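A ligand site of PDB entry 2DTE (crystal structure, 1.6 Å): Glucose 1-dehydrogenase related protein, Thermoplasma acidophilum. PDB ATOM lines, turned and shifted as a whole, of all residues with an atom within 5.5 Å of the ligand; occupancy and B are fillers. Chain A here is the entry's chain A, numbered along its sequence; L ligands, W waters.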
ATOM      1  N   THR A  14       9.224   1.822  22.405  1.00  0.00           N
ATOM      2  CA  THR A  14       8.384   0.690  22.024  1.00  0.00           C
ATOM      3  C   THR A  14       7.142   1.186  21.289  1.00  0.00           C
ATOM      4  O   THR A  14       6.645   2.284  21.574  1.00  0.00           O
ATOM      5  CB  THR A  14       7.950  -0.161  23.246  1.00  0.00           C
ATOM      6  OG1 THR A  14       7.018   0.562  24.058  1.00  0.00           O
ATOM      7  CG2 THR A  14       9.156  -0.543  24.084  1.00  0.00           C
ATOM      8  N   GLY A  15       6.670   0.397  20.326  1.00  0.00           N
ATOM      9  CA  GLY A  15       5.501   0.778  19.565  1.00  0.00           C
ATOM     10  C   GLY A  15       5.712   2.057  18.764  1.00  0.00           C
ATOM     11  O   GLY A  15       4.815   2.908  18.718  1.00  0.00           O
ATOM     12  N   ALA A  16       6.875   2.190  18.142  1.00  0.00           N
ATOM     13  CA  ALA A  16       7.196   3.393  17.372  1.00  0.00           C
ATOM     14  C   ALA A  16       7.058   3.228  15.861  1.00  0.00           C
ATOM     15  O   ALA A  16       7.674   3.979  15.101  1.00  0.00           O
ATOM     16  CB  ALA A  16       8.601   3.858  17.716  1.00  0.00           C
ATOM     17  N   SER A  17       6.232   2.275  15.427  1.00  0.00           N
ATOM     18  CA  SER A  17       6.030   2.061  14.002  1.00  0.00           C
ATOM     19  C   SER A  17       4.862   2.881  13.444  1.00  0.00           C
ATOM     20  O   SER A  17       4.624   2.900  12.235  1.00  0.00           O
ATOM     21  CB  SER A  17       5.822   0.571  13.706  1.00  0.00           C
ATOM     22  OG  SER A  17       4.896  -0.017  14.604  1.00  0.00           O
ATOM     23  N   MET A  18       4.146   3.570  14.331  1.00  0.00           N
ATOM     24  CA  MET A  18       3.023   4.421  13.937  1.00  0.00           C
ATOM     25  C   MET A  18       2.551   5.283  15.113  1.00  0.00           C
ATOM     26  O   MET A  18       3.056   5.127  16.220  1.00  0.00           O
ATOM     27  CB  MET A  18       1.844   3.562  13.467  1.00  0.00           C
ATOM     28  CG  MET A  18       1.223   2.706  14.562  1.00  0.00           C
ATOM     29  SD  MET A  18      -0.074   1.604  13.963  1.00  0.00           S
ATOM     30  CE  MET A  18       0.914   0.261  13.276  1.00  0.00           C
ATOM     31  N   GLY A  19       1.616   6.184  14.838  1.00  0.00           N
ATOM     32  CA  GLY A  19       1.049   7.041  15.866  1.00  0.00           C
ATOM     33  C   GLY A  19       2.005   7.832  16.746  1.00  0.00           C
ATOM     34  O   GLY A  19       3.012   8.358  16.291  1.00  0.00           O
ATOM     35  N   ILE A  20       1.661   7.912  18.028  1.00  0.00           N
ATOM     36  CA  ILE A  20       2.476   8.646  18.986  1.00  0.00           C
ATOM     37  C   ILE A  20       3.902   8.136  19.057  1.00  0.00           C
ATOM     38  O   ILE A  20       4.838   8.935  19.127  1.00  0.00           O
ATOM     39  CB  ILE A  20       1.822   8.590  20.391  1.00  0.00           C
ATOM     40  CG1 ILE A  20       0.513   9.391  20.357  1.00  0.00           C
ATOM     41  CG2 ILE A  20       2.777   9.132  21.442  1.00  0.00           C
ATOM     42  CD1 ILE A  20      -0.325   9.247  21.615  1.00  0.00           C
ATOM     43  N   GLY A  21       4.070   6.820  19.030  1.00  0.00           N
ATOM     44  CA  GLY A  21       5.401   6.230  19.097  1.00  0.00           C
ATOM     45  C   GLY A  21       6.278   6.632  17.922  1.00  0.00           C
ATOM     46  O   GLY A  21       7.479   6.858  18.083  1.00  0.00           O
ATOM     47  N   LEU A  38      11.007  -0.851  19.043  1.00  0.00           N
ATOM     48  CA  LEU A  38      10.723  -2.241  19.387  1.00  0.00           C
ATOM     49  C   LEU A  38       9.220  -2.356  19.185  1.00  0.00           C
ATOM     50  O   LEU A  38       8.441  -1.811  19.963  1.00  0.00           O
ATOM     51  CB  LEU A  38      11.077  -2.572  20.837  1.00  0.00           C
ATOM     52  CG  LEU A  38      12.550  -2.526  21.217  1.00  0.00           C
ATOM     53  CD1 LEU A  38      12.700  -3.085  22.630  1.00  0.00           C
ATOM     54  CD2 LEU A  38      13.386  -3.354  20.221  1.00  0.00           C
ATOM     55  N   SER A  39       8.807  -3.008  18.100  1.00  0.00           N
ATOM     56  CA  SER A  39       7.381  -3.162  17.853  1.00  0.00           C
ATOM     57  C   SER A  39       7.094  -4.352  16.953  1.00  0.00           C
ATOM     58  O   SER A  39       8.010  -4.985  16.453  1.00  0.00           O
ATOM     59  CB  SER A  39       6.795  -1.884  17.229  1.00  0.00           C
ATOM     60  OG  SER A  39       7.150  -1.750  15.860  1.00  0.00           O
ATOM     61  N   ILE A  40       5.808  -4.616  16.758  1.00  0.00           N
ATOM     62  CA  ILE A  40       5.370  -5.738  15.927  1.00  0.00           C
ATOM     63  C   ILE A  40       4.931  -5.312  14.527  1.00  0.00           C
ATOM     64  O   ILE A  40       4.163  -6.019  13.876  1.00  0.00           O
ATOM     65  CB  ILE A  40       4.222  -6.512  16.597  1.00  0.00           C
ATOM     66  CG1 ILE A  40       3.074  -5.551  16.937  1.00  0.00           C
ATOM     67  CG2 ILE A  40       4.749  -7.250  17.814  1.00  0.00           C
ATOM     68  CD1 ILE A  40       1.848  -6.223  17.533  1.00  0.00           C
ATOM     69  N   HIS A  41       5.407  -4.163  14.081  1.00  0.00           N
ATOM     70  CA  HIS A  41       5.059  -3.659  12.761  1.00  0.00           C
ATOM     71  C   HIS A  41       6.263  -2.955  12.151  1.00  0.00           C
ATOM     72  O   HIS A  41       6.952  -2.200  12.836  1.00  0.00           O
ATOM     73  CB  HIS A  41       3.866  -2.706  12.841  1.00  0.00           C
ATOM     74  CG  HIS A  41       3.400  -2.196  11.515  1.00  0.00           C
ATOM     75  ND1 HIS A  41       4.163  -1.360  10.720  1.00  0.00           N
ATOM     76  CD2 HIS A  41       2.254  -2.412  10.831  1.00  0.00           C
ATOM     77  CE1 HIS A  41       3.503  -1.091   9.608  1.00  0.00           C
ATOM     78  NE2 HIS A  41       2.341  -1.710   9.651  1.00  0.00           N
ATOM     79  N   CYS A  53       9.625  -7.009  17.737  1.00  0.00           N
ATOM     80  CA  CYS A  53       9.565  -7.367  19.133  1.00  0.00           C
ATOM     81  C   CYS A  53       8.183  -7.186  19.725  1.00  0.00           C
ATOM     82  O   CYS A  53       7.613  -6.092  19.661  1.00  0.00           O
ATOM     83  CB  CYS A  53      10.570  -6.523  19.913  1.00  0.00           C
ATOM     84  SG  CYS A  53      10.666  -6.890  21.655  1.00  0.00           S
ATOM     85  N   ASP A  54       7.641  -8.275  20.282  1.00  0.00           N
ATOM     86  CA  ASP A  54       6.330  -8.295  20.935  1.00  0.00           C
ATOM     87  C   ASP A  54       6.619  -8.024  22.411  1.00  0.00           C
ATOM     88  O   ASP A  54       7.265  -8.839  23.078  1.00  0.00           O
ATOM     89  CB  ASP A  54       5.700  -9.690  20.749  1.00  0.00           C
ATOM     90  CG  ASP A  54       4.338  -9.814  21.376  1.00  0.00           C
ATOM     91  OD1 ASP A  54       3.998  -9.009  22.273  1.00  0.00           O
ATOM     92  OD2 ASP A  54       3.601 -10.738  20.987  1.00  0.00           O
ATOM     93  N   VAL A  55       6.170  -6.873  22.919  1.00  0.00           N
ATOM     94  CA  VAL A  55       6.441  -6.541  24.309  1.00  0.00           C
ATOM     95  C   VAL A  55       5.835  -7.473  25.359  1.00  0.00           C
ATOM     96  O   VAL A  55       6.217  -7.398  26.523  1.00  0.00           O
ATOM     97  CB  VAL A  55       6.016  -5.073  24.636  1.00  0.00           C
ATOM     98  CG1 VAL A  55       6.774  -4.111  23.725  1.00  0.00           C
ATOM     99  CG2 VAL A  55       4.511  -4.892  24.465  1.00  0.00           C
ATOM    100  N   THR A  56       4.922  -8.348  24.958  1.00  0.00           N
ATOM    101  CA  THR A  56       4.342  -9.296  25.919  1.00  0.00           C
ATOM    102  C   THR A  56       5.214 -10.542  26.045  1.00  0.00           C
ATOM    103  O   THR A  56       4.946 -11.408  26.871  1.00  0.00           O
ATOM    104  CB  THR A  56       2.905  -9.733  25.540  1.00  0.00           C
ATOM    105  OG1 THR A  56       2.921 -10.495  24.320  1.00  0.00           O
ATOM    106  CG2 THR A  56       2.005  -8.509  25.381  1.00  0.00           C
ATOM    107  N   ASN A  81       5.807   2.904  25.177  1.00  0.00           N
ATOM    108  CA  ASN A  81       4.661   3.486  24.490  1.00  0.00           C
ATOM    109  C   ASN A  81       3.682   2.471  23.897  1.00  0.00           C
ATOM    110  O   ASN A  81       2.488   2.742  23.784  1.00  0.00           O
ATOM    111  CB  ASN A  81       5.188   4.420  23.392  1.00  0.00           C
ATOM    112  CG  ASN A  81       4.134   4.861  22.405  1.00  0.00           C
ATOM    113  OD1 ASN A  81       3.430   5.849  22.607  1.00  0.00           O
ATOM    114  ND2 ASN A  81       4.019   4.118  21.312  1.00  0.00           N
ATOM    115  N   ALA A  82       4.175   1.304  23.500  1.00  0.00           N
ATOM    116  CA  ALA A  82       3.328   0.290  22.886  1.00  0.00           C
ATOM    117  C   ALA A  82       2.081   0.049  23.721  1.00  0.00           C
ATOM    118  O   ALA A  82       2.155  -0.169  24.930  1.00  0.00           O
ATOM    119  CB  ALA A  82       4.106  -1.023  22.717  1.00  0.00           C
ATOM    120  N   GLY A  83       0.918   0.106  23.079  1.00  0.00           N
ATOM    121  CA  GLY A  83      -0.305  -0.113  23.821  1.00  0.00           C
ATOM    122  C   GLY A  83      -1.453  -0.359  22.884  1.00  0.00           C
ATOM    123  O   GLY A  83      -1.383  -0.014  21.710  1.00  0.00           O
ATOM    124  N   ILE A  84      -2.507  -0.976  23.413  1.00  0.00           N
ATOM    125  CA  ILE A  84      -3.688  -1.273  22.633  1.00  0.00           C
ATOM    126  C   ILE A  84      -4.947  -0.923  23.422  1.00  0.00           C
ATOM    127  O   ILE A  84      -4.901  -0.693  24.632  1.00  0.00           O
ATOM    128  CB  ILE A  84      -3.772  -2.788  22.304  1.00  0.00           C
ATOM    129  CG1 ILE A  84      -3.698  -3.617  23.583  1.00  0.00           C
ATOM    130  CG2 ILE A  84      -2.624  -3.168  21.377  1.00  0.00           C
ATOM    131  CD1 ILE A  84      -4.040  -5.093  23.401  1.00  0.00           C
ATOM    132  N   VAL A 104      -0.227  -6.279  27.401  1.00  0.00           N
ATOM    133  CA  VAL A 104       0.491  -5.325  26.560  1.00  0.00           C
ATOM    134  C   VAL A 104       0.755  -4.000  27.276  1.00  0.00           C
ATOM    135  O   VAL A 104       1.891  -3.548  27.389  1.00  0.00           O
ATOM    136  CB  VAL A 104      -0.298  -4.977  25.277  1.00  0.00           C
ATOM    137  CG1 VAL A 104       0.461  -3.936  24.468  1.00  0.00           C
ATOM    138  CG2 VAL A 104      -0.529  -6.237  24.436  1.00  0.00           C
ATOM    139  N   ASN A 105      -0.314  -3.405  27.798  1.00  0.00           N
ATOM    140  CA  ASN A 105      -0.250  -2.078  28.417  1.00  0.00           C
ATOM    141  C   ASN A 105       0.512  -1.931  29.724  1.00  0.00           C
ATOM    142  O   ASN A 105       1.072  -0.868  29.991  1.00  0.00           O
ATOM    143  CB  ASN A 105      -1.666  -1.540  28.575  1.00  0.00           C
ATOM    144  CG  ASN A 105      -2.329  -1.259  27.250  1.00  0.00           C
ATOM    145  OD1 ASN A 105      -1.810  -1.619  26.196  1.00  0.00           O
ATOM    146  ND2 ASN A 105      -3.498  -0.622  27.285  1.00  0.00           N
ATOM    147  N   TYR A 109       5.395  -2.773  29.659  1.00  0.00           N
ATOM    148  CA  TYR A 109       6.195  -1.712  30.288  1.00  0.00           C
ATOM    149  C   TYR A 109       7.088  -2.302  31.370  1.00  0.00           C
ATOM    150  O   TYR A 109       8.233  -1.887  31.554  1.00  0.00           O
ATOM    151  CB  TYR A 109       5.278  -0.648  30.905  1.00  0.00           C
ATOM    152  CG  TYR A 109       4.644   0.329  29.935  1.00  0.00           C
ATOM    153  CD1 TYR A 109       4.353  -0.035  28.618  1.00  0.00           C
ATOM    154  CD2 TYR A 109       4.294   1.618  30.353  1.00  0.00           C
ATOM    155  CE1 TYR A 109       3.729   0.864  27.740  1.00  0.00           C
ATOM    156  CE2 TYR A 109       3.664   2.523  29.481  1.00  0.00           C
ATOM    157  CZ  TYR A 109       3.383   2.134  28.178  1.00  0.00           C
ATOM    158  OH  TYR A 109       2.704   2.994  27.336  1.00  0.00           O
ATOM    159  N   ILE A 131       4.280   6.129  28.629  1.00  0.00           N
ATOM    160  CA  ILE A 131       3.080   6.797  28.133  1.00  0.00           C
ATOM    161  C   ILE A 131       1.851   6.182  28.801  1.00  0.00           C
ATOM    162  O   ILE A 131       1.547   4.999  28.608  1.00  0.00           O
ATOM    163  CB  ILE A 131       2.917   6.688  26.601  1.00  0.00           C
ATOM    164  CG1 ILE A 131       4.193   7.156  25.882  1.00  0.00           C
ATOM    165  CG2 ILE A 131       1.719   7.534  26.152  1.00  0.00           C
ATOM    166  CD1 ILE A 131       4.615   8.595  26.207  1.00  0.00           C
ATOM    167  N   SER A 132       1.199   6.967  29.655  1.00  0.00           N
ATOM    168  CA  SER A 132      -0.021   6.509  30.331  1.00  0.00           C
ATOM    169  C   SER A 132      -1.201   7.083  29.546  1.00  0.00           C
ATOM    170  O   SER A 132      -1.329   6.825  28.358  1.00  0.00           O
ATOM    171  CB  SER A 132      -0.054   6.986  31.789  1.00  0.00           C
ATOM    172  OG  SER A 132      -1.237   6.561  32.449  1.00  0.00           O
ATOM    173  N   SER A 133      -2.051   7.882  30.186  1.00  0.00           N
ATOM    174  CA  SER A 133      -3.221   8.465  29.525  1.00  0.00           C
ATOM    175  C   SER A 133      -3.863   9.446  30.479  1.00  0.00           C
ATOM    176  O   SER A 133      -3.624   9.385  31.678  1.00  0.00           O
ATOM    177  CB  SER A 133      -4.256   7.383  29.225  1.00  0.00           C
ATOM    178  OG  SER A 133      -5.462   7.925  28.710  1.00  0.00           O
ATOM    179  N   VAL A 134      -4.681  10.351  29.936  1.00  0.00           N
ATOM    180  CA  VAL A 134      -5.428  11.283  30.772  1.00  0.00           C
ATOM    181  C   VAL A 134      -6.372  10.388  31.584  1.00  0.00           C
ATOM    182  O   VAL A 134      -6.858  10.792  32.641  1.00  0.00           O
ATOM    183  CB  VAL A 134      -6.239  12.298  29.908  1.00  0.00           C
ATOM    184  CG1 VAL A 134      -7.374  11.586  29.173  1.00  0.00           C
ATOM    185  CG2 VAL A 134      -6.777  13.439  30.771  1.00  0.00           C
ATOM    186  N   TYR A 146      -8.503  -1.131  29.767  1.00  0.00           N
ATOM    187  CA  TYR A 146      -7.646  -0.040  29.363  1.00  0.00           C
ATOM    188  C   TYR A 146      -7.388   0.926  30.512  1.00  0.00           C
ATOM    189  O   TYR A 146      -6.242   1.279  30.814  1.00  0.00           O
ATOM    190  CB  TYR A 146      -8.266   0.722  28.190  1.00  0.00           C
ATOM    191  CG  TYR A 146      -7.373   1.827  27.663  1.00  0.00           C
ATOM    192  CD1 TYR A 146      -6.306   1.524  26.807  1.00  0.00           C
ATOM    193  CD2 TYR A 146      -7.573   3.162  28.020  1.00  0.00           C
ATOM    194  CE1 TYR A 146      -5.470   2.531  26.320  1.00  0.00           C
ATOM    195  CE2 TYR A 146      -6.735   4.174  27.547  1.00  0.00           C
ATOM    196  CZ  TYR A 146      -5.682   3.847  26.700  1.00  0.00           C
ATOM    197  OH  TYR A 146      -4.857   4.833  26.207  1.00  0.00           O
ATOM    198  N   LYS A 150      -3.850   1.759  32.526  1.00  0.00           N
ATOM    199  CA  LYS A 150      -3.211   3.077  32.540  1.00  0.00           C
ATOM    200  C   LYS A 150      -2.966   3.593  33.950  1.00  0.00           C
ATOM    201  O   LYS A 150      -2.001   4.310  34.192  1.00  0.00           O
ATOM    202  CB  LYS A 150      -4.012   4.067  31.690  1.00  0.00           C
ATOM    203  CG  LYS A 150      -3.979   3.717  30.183  1.00  0.00           C
ATOM    204  CD  LYS A 150      -2.514   3.604  29.721  1.00  0.00           C
ATOM    205  CE  LYS A 150      -2.382   3.426  28.203  1.00  0.00           C
ATOM    206  NZ  LYS A 150      -0.942   3.441  27.779  1.00  0.00           N
ATOM    207  N   PRO A 175      -1.498  11.762  27.948  1.00  0.00           N
ATOM    208  CA  PRO A 175      -2.204  12.465  26.867  1.00  0.00           C
ATOM    209  C   PRO A 175      -3.713  12.248  26.856  1.00  0.00           C
ATOM    210  O   PRO A 175      -4.217  11.191  27.277  1.00  0.00           O
ATOM    211  CB  PRO A 175      -1.569  11.897  25.593  1.00  0.00           C
ATOM    212  CG  PRO A 175      -0.349  11.106  26.058  1.00  0.00           C
ATOM    213  CD  PRO A 175      -0.786  10.586  27.422  1.00  0.00           C
ATOM    214  N   ALA A 176      -4.435  13.254  26.364  1.00  0.00           N
ATOM    215  CA  ALA A 176      -5.884  13.133  26.193  1.00  0.00           C
ATOM    216  C   ALA A 176      -6.025  12.681  24.730  1.00  0.00           C
ATOM    217  O   ALA A 176      -5.167  11.946  24.227  1.00  0.00           O
ATOM    218  CB  ALA A 176      -6.589  14.477  26.422  1.00  0.00           C
ATOM    219  N   THR A 177      -7.070  13.097  24.022  1.00  0.00           N
ATOM    220  CA  THR A 177      -7.233  12.624  22.652  1.00  0.00           C
ATOM    221  C   THR A 177      -6.174  13.156  21.692  1.00  0.00           C
ATOM    222  O   THR A 177      -6.018  14.359  21.518  1.00  0.00           O
ATOM    223  CB  THR A 177      -8.627  12.966  22.104  1.00  0.00           C
ATOM    224  OG1 THR A 177      -9.614  12.574  23.061  1.00  0.00           O
ATOM    225  CG2 THR A 177      -8.888  12.213  20.811  1.00  0.00           C
ATOM    226  N   ILE A 178      -5.467  12.235  21.032  1.00  0.00           N
ATOM    227  CA  ILE A 178      -4.417  12.610  20.093  1.00  0.00           C
ATOM    228  C   ILE A 178      -4.707  12.016  18.700  1.00  0.00           C
ATOM    229  O   ILE A 178      -5.171  10.885  18.583  1.00  0.00           O
ATOM    230  CB  ILE A 178      -3.028  12.086  20.581  1.00  0.00           C
ATOM    231  CG1 ILE A 178      -2.766  12.535  22.033  1.00  0.00           C
ATOM    232  CG2 ILE A 178      -1.932  12.570  19.645  1.00  0.00           C
ATOM    233  CD1 ILE A 178      -2.756  14.046  22.248  1.00  0.00           C
ATOM    234  N   ASP A 179      -4.437  12.788  17.649  1.00  0.00           N
ATOM    235  CA  ASP A 179      -4.705  12.318  16.288  1.00  0.00           C
ATOM    236  C   ASP A 179      -3.740  11.180  15.913  1.00  0.00           C
ATOM    237  O   ASP A 179      -2.606  11.430  15.506  1.00  0.00           O
ATOM    238  CB  ASP A 179      -4.544  13.487  15.298  1.00  0.00           C
ATOM    239  CG  ASP A 179      -5.202  13.205  13.958  1.00  0.00           C
ATOM    240  OD1 ASP A 179      -5.433  12.016  13.643  1.00  0.00           O
ATOM    241  OD2 ASP A 179      -5.494  14.181  13.229  1.00  0.00           O
ATOM    242  N   THR A 180      -4.212   9.949  16.048  1.00  0.00           N
ATOM    243  CA  THR A 180      -3.402   8.755  15.738  1.00  0.00           C
ATOM    244  C   THR A 180      -4.287   7.662  15.148  1.00  0.00           C
ATOM    245  O   THR A 180      -5.502   7.787  15.100  1.00  0.00           O
ATOM    246  CB  THR A 180      -2.753   8.148  16.999  1.00  0.00           C
ATOM    247  OG1 THR A 180      -3.766   7.518  17.788  1.00  0.00           O
ATOM    248  CG2 THR A 180      -2.076   9.218  17.832  1.00  0.00           C
ATOM    249  N   PRO A 181      -3.668   6.556  14.689  1.00  0.00           N
ATOM    250  CA  PRO A 181      -4.456   5.461  14.114  1.00  0.00           C
ATOM    251  C   PRO A 181      -5.467   4.916  15.109  1.00  0.00           C
ATOM    252  O   PRO A 181      -6.610   4.639  14.760  1.00  0.00           O
ATOM    253  CB  PRO A 181      -3.389   4.430  13.757  1.00  0.00           C
ATOM    254  CG  PRO A 181      -2.232   5.278  13.370  1.00  0.00           C
ATOM    255  CD  PRO A 181      -2.227   6.341  14.452  1.00  0.00           C
ATOM    256  N   LEU A 182      -5.043   4.769  16.361  1.00  0.00           N
ATOM    257  CA  LEU A 182      -5.918   4.251  17.409  1.00  0.00           C
ATOM    258  C   LEU A 182      -7.183   5.109  17.545  1.00  0.00           C
ATOM    259  O   LEU A 182      -8.293   4.585  17.624  1.00  0.00           O
ATOM    260  CB  LEU A 182      -5.166   4.199  18.759  1.00  0.00           C
ATOM    261  CG  LEU A 182      -5.850   3.567  19.979  1.00  0.00           C
ATOM    262  CD1 LEU A 182      -4.798   3.282  21.043  1.00  0.00           C
ATOM    263  CD2 LEU A 182      -6.928   4.489  20.532  1.00  0.00           C
ATOM    264  N   VAL A 183      -7.004   6.432  17.546  1.00  0.00           N
ATOM    265  CA  VAL A 183      -8.139   7.347  17.674  1.00  0.00           C
ATOM    266  C   VAL A 183      -8.990   7.401  16.398  1.00  0.00           C
ATOM    267  O   VAL A 183     -10.216   7.471  16.468  1.00  0.00           O
ATOM    268  CB  VAL A 183      -7.660   8.774  18.053  1.00  0.00           C
ATOM    269  CG1 VAL A 183      -8.795   9.758  17.903  1.00  0.00           C
ATOM    270  CG2 VAL A 183      -7.162   8.779  19.477  1.00  0.00           C
HETATM  271  P1  LIG L   1      -1.287   3.106  17.798  1.00  0.00           P
HETATM  272  O1  LIG L   1      -2.149   1.923  17.706  1.00  0.00           O
HETATM  273  O2  LIG L   1      -1.320   3.982  16.602  1.00  0.00           O
HETATM  274  O3  LIG L   1       0.251   2.712  17.979  1.00  0.00           O
HETATM  275  C1  LIG L   1       0.566   1.555  18.809  1.00  0.00           C
HETATM  276  C2  LIG L   1       1.936   1.003  18.550  1.00  0.00           C
HETATM  277  O4  LIG L   1       1.984  -0.118  19.477  1.00  0.00           O
HETATM  278  C3  LIG L   1       2.101   0.377  17.157  1.00  0.00           C
HETATM  279  O5  LIG L   1       3.336   0.865  16.574  1.00  0.00           O
HETATM  280  C4  LIG L   1       2.119  -1.129  17.439  1.00  0.00           C
HETATM  281  O6  LIG L   1       2.949  -1.878  16.509  1.00  0.00           O
HETATM  282  C5  LIG L   1       2.637  -1.187  18.858  1.00  0.00           C
HETATM  283  N1  LIG L   1       2.231  -2.416  19.537  1.00  0.00           N
HETATM  284  C6  LIG L   1       0.957  -2.844  19.882  1.00  0.00           C
HETATM  285  N2  LIG L   1       0.949  -4.034  20.532  1.00  0.00           N
HETATM  286  C7  LIG L   1       2.309  -4.375  20.589  1.00  0.00           C
HETATM  287  C8  LIG L   1       2.995  -5.510  21.136  1.00  0.00           C
HETATM  288  N3  LIG L   1       2.375  -6.531  21.744  1.00  0.00           N
HETATM  289  N4  LIG L   1       4.390  -5.513  21.018  1.00  0.00           N
HETATM  290  C9  LIG L   1       5.022  -4.458  20.390  1.00  0.00           C
HETATM  291  N5  LIG L   1       4.482  -3.380  19.854  1.00  0.00           N
HETATM  292  C10 LIG L   1       3.111  -3.376  19.975  1.00  0.00           C
HETATM  293  O7  LIG L   1      -1.680   3.899  19.097  1.00  0.00           O
HETATM  294  P2  LIG L   1      -1.202   5.280  19.747  1.00  0.00           P
HETATM  295  O8  LIG L   1      -2.461   6.099  19.737  1.00  0.00           O
HETATM  296  O9  LIG L   1      -0.135   5.876  18.922  1.00  0.00           O
HETATM  297  O10 LIG L   1      -0.873   5.110  21.284  1.00  0.00           O
HETATM  298  C11 LIG L   1       0.486   5.002  21.724  1.00  0.00           C
HETATM  299  C12 LIG L   1       0.461   4.967  23.234  1.00  0.00           C
HETATM  300  O11 LIG L   1      -0.151   6.214  23.684  1.00  0.00           O
HETATM  301  C13 LIG L   1      -0.345   3.838  23.914  1.00  0.00           C
HETATM  302  O12 LIG L   1       0.270   3.410  25.144  1.00  0.00           O
HETATM  303  C14 LIG L   1      -1.686   4.512  24.151  1.00  0.00           C
HETATM  304  O13 LIG L   1      -2.422   3.779  25.172  1.00  0.00           O
HETATM  305  C15 LIG L   1      -1.218   5.892  24.548  1.00  0.00           C
HETATM  306  N6  LIG L   1      -2.257   6.935  24.499  1.00  0.00           N
HETATM  307  C16 LIG L   1      -2.794   7.241  23.235  1.00  0.00           C
HETATM  308  C17 LIG L   1      -3.774   8.232  23.202  1.00  0.00           C
HETATM  309  C18 LIG L   1      -4.446   8.683  21.920  1.00  0.00           C
HETATM  310  O14 LIG L   1      -5.320   9.553  21.983  1.00  0.00           O
HETATM  311  N7  LIG L   1      -4.079   8.138  20.739  1.00  0.00           N
HETATM  312  C19 LIG L   1      -4.215   8.906  24.411  1.00  0.00           C
HETATM  313  C20 LIG L   1      -3.589   8.499  25.618  1.00  0.00           C
HETATM  314  C21 LIG L   1      -2.630   7.532  25.738  1.00  0.00           C
HETATM  315  O   HOH W   1       2.333   4.583  19.048  1.00  0.00           O
HETATM  316  O   HOH W   2      -2.897   0.024  19.430  1.00  0.00           O
HETATM  317  O   HOH W   3      -0.763  -6.294  20.591  1.00  0.00           O
HETATM  318  O   HOH W   4      -4.357   1.183  16.072  1.00  0.00           O
HETATM  319  O   HOH W   5      -6.376   7.111  26.291  1.00  0.00           O
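An oxygen (O2) of the ligand lies close to the side-chain sulfur (SD) of Met 18 (3.8 Å). O of Ala 176 lies close to O14 of the ligand (3.3 Å). Residues that only touch the ligand: Gly 19, Ser 39, Ile 40, His 41, Cys 53, Ala 82, Gly 83, Ile 84, Val 104, Ile 131, Ser 132, Ser 133, Pro 175, Thr 177, Pro 181, Leu 182 and Val 183. Within 4 Å of the ligand: Gly 15, Ser 17, Met 18, Gly 19, Ile 20, Ser 39, Ile 40, His 41, Cys 53, Asp 54, Val 55, Asn 81, Ala 82, Gly 83, Ile 84, Val 104, Tyr 109, Ile 131, Ser 132, Ser 133, Tyr 146, Lys 150, Pro 175, Ala 176, Thr 177, Ile 178, Thr 180, Pro 181, Leu 182 and Val 183. The nearest printed residue that does not touch the ligand is Ala 16 (4.1 Å).
Water W2 lies within hydrogen-bond range of O1 of the ligand and O of Gly 83. Water W1 lies within hydrogen-bond range of an oxygen (O9) of the ligand (2.8 Å), the backbone NH of Gly 21 (2.8 Å), the side-chain amide nitrogen of Asn 81 (2.9 Å), the backbone carbonyl oxygen of Met 18 (3.0 Å) and the backbone carbonyl oxygen of Gly 15 (3.0 Å). Water W5 lies within hydrogen-bond range of the side-chain hydroxyl of Ser 133 and the side-chain hydroxyl of Tyr 146.
N of Ser 17 lies within hydrogen-bond range of O5 of the ligand (3.4 Å). The side-chain hydroxyl (OG) of Ser 17 sits at hydrogen-bond distance from an oxygen (O5) of the ligand (2.7 Å). An oxygen (O12) of the ligand lies within hydrogen-bond range of the backbone carbonyl oxygen (O) of Asn 81 (2.7 Å). The side-chain hydroxyl (OG1) of Thr 180 sits at hydrogen-bond distance from an oxygen (O8) of the ligand, 2.7 Å away. OH of Tyr 146 is in hydrogen-bond range of O13 of the ligand (2.8 Å). N of Ile 178 is in hydrogen-bond range of O14 of the ligand, at 2.8 Å. An oxygen (O9) of the ligand lies within hydrogen-bond range of the backbone NH of Ile 20 (2.9 Å). An oxygen (O12) of the ligand lies within hydrogen-bond range of the side-chain amino group of Lys 150 (2.9 Å). The backbone NH of Val 55 lies within hydrogen-bond range of a nitrogen (N4) of the ligand (2.9 Å). The side-chain carboxylate of Asp 54 sits at hydrogen-bond distance from a nitrogen (N3) of the ligand (3.0 Å). The side-chain hydroxyl of Tyr 109 lies within hydrogen-bond range of an oxygen (O12) of the ligand (3.3 Å). O of Gly 15 sits at hydrogen-bond distance from O5 of the ligand (3.3 Å).
OG1 of Thr 14 lies within hydrogen-bond range of N of Asn 81. OG1 of Thr 180 sits at hydrogen-bond distance from N of Val 183, at 3.4 Å. The side-chain hydroxyl of Thr 180 lies close to the backbone NH of Leu 182. The side-chain hydroxyl (OG) of Ser 132 sits at hydrogen-bond distance from the backbone carbonyl oxygen (O) of Lys 150 (2.9 Å). The side-chain amino group (NZ) of Lys 150 sits at hydrogen-bond distance from the backbone carbonyl oxygen (O) of Ile 131. OG1 of Thr 56 is in hydrogen-bond range of OD1 of Asp 54 (2.7 Å). The backbone carbonyl oxygen of Leu 38 sits at hydrogen-bond distance from the backbone NH of Gly 15, at 2.9 Å. OG of Ser 39 lies within hydrogen-bond range of O of His 41 (3.1 Å).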
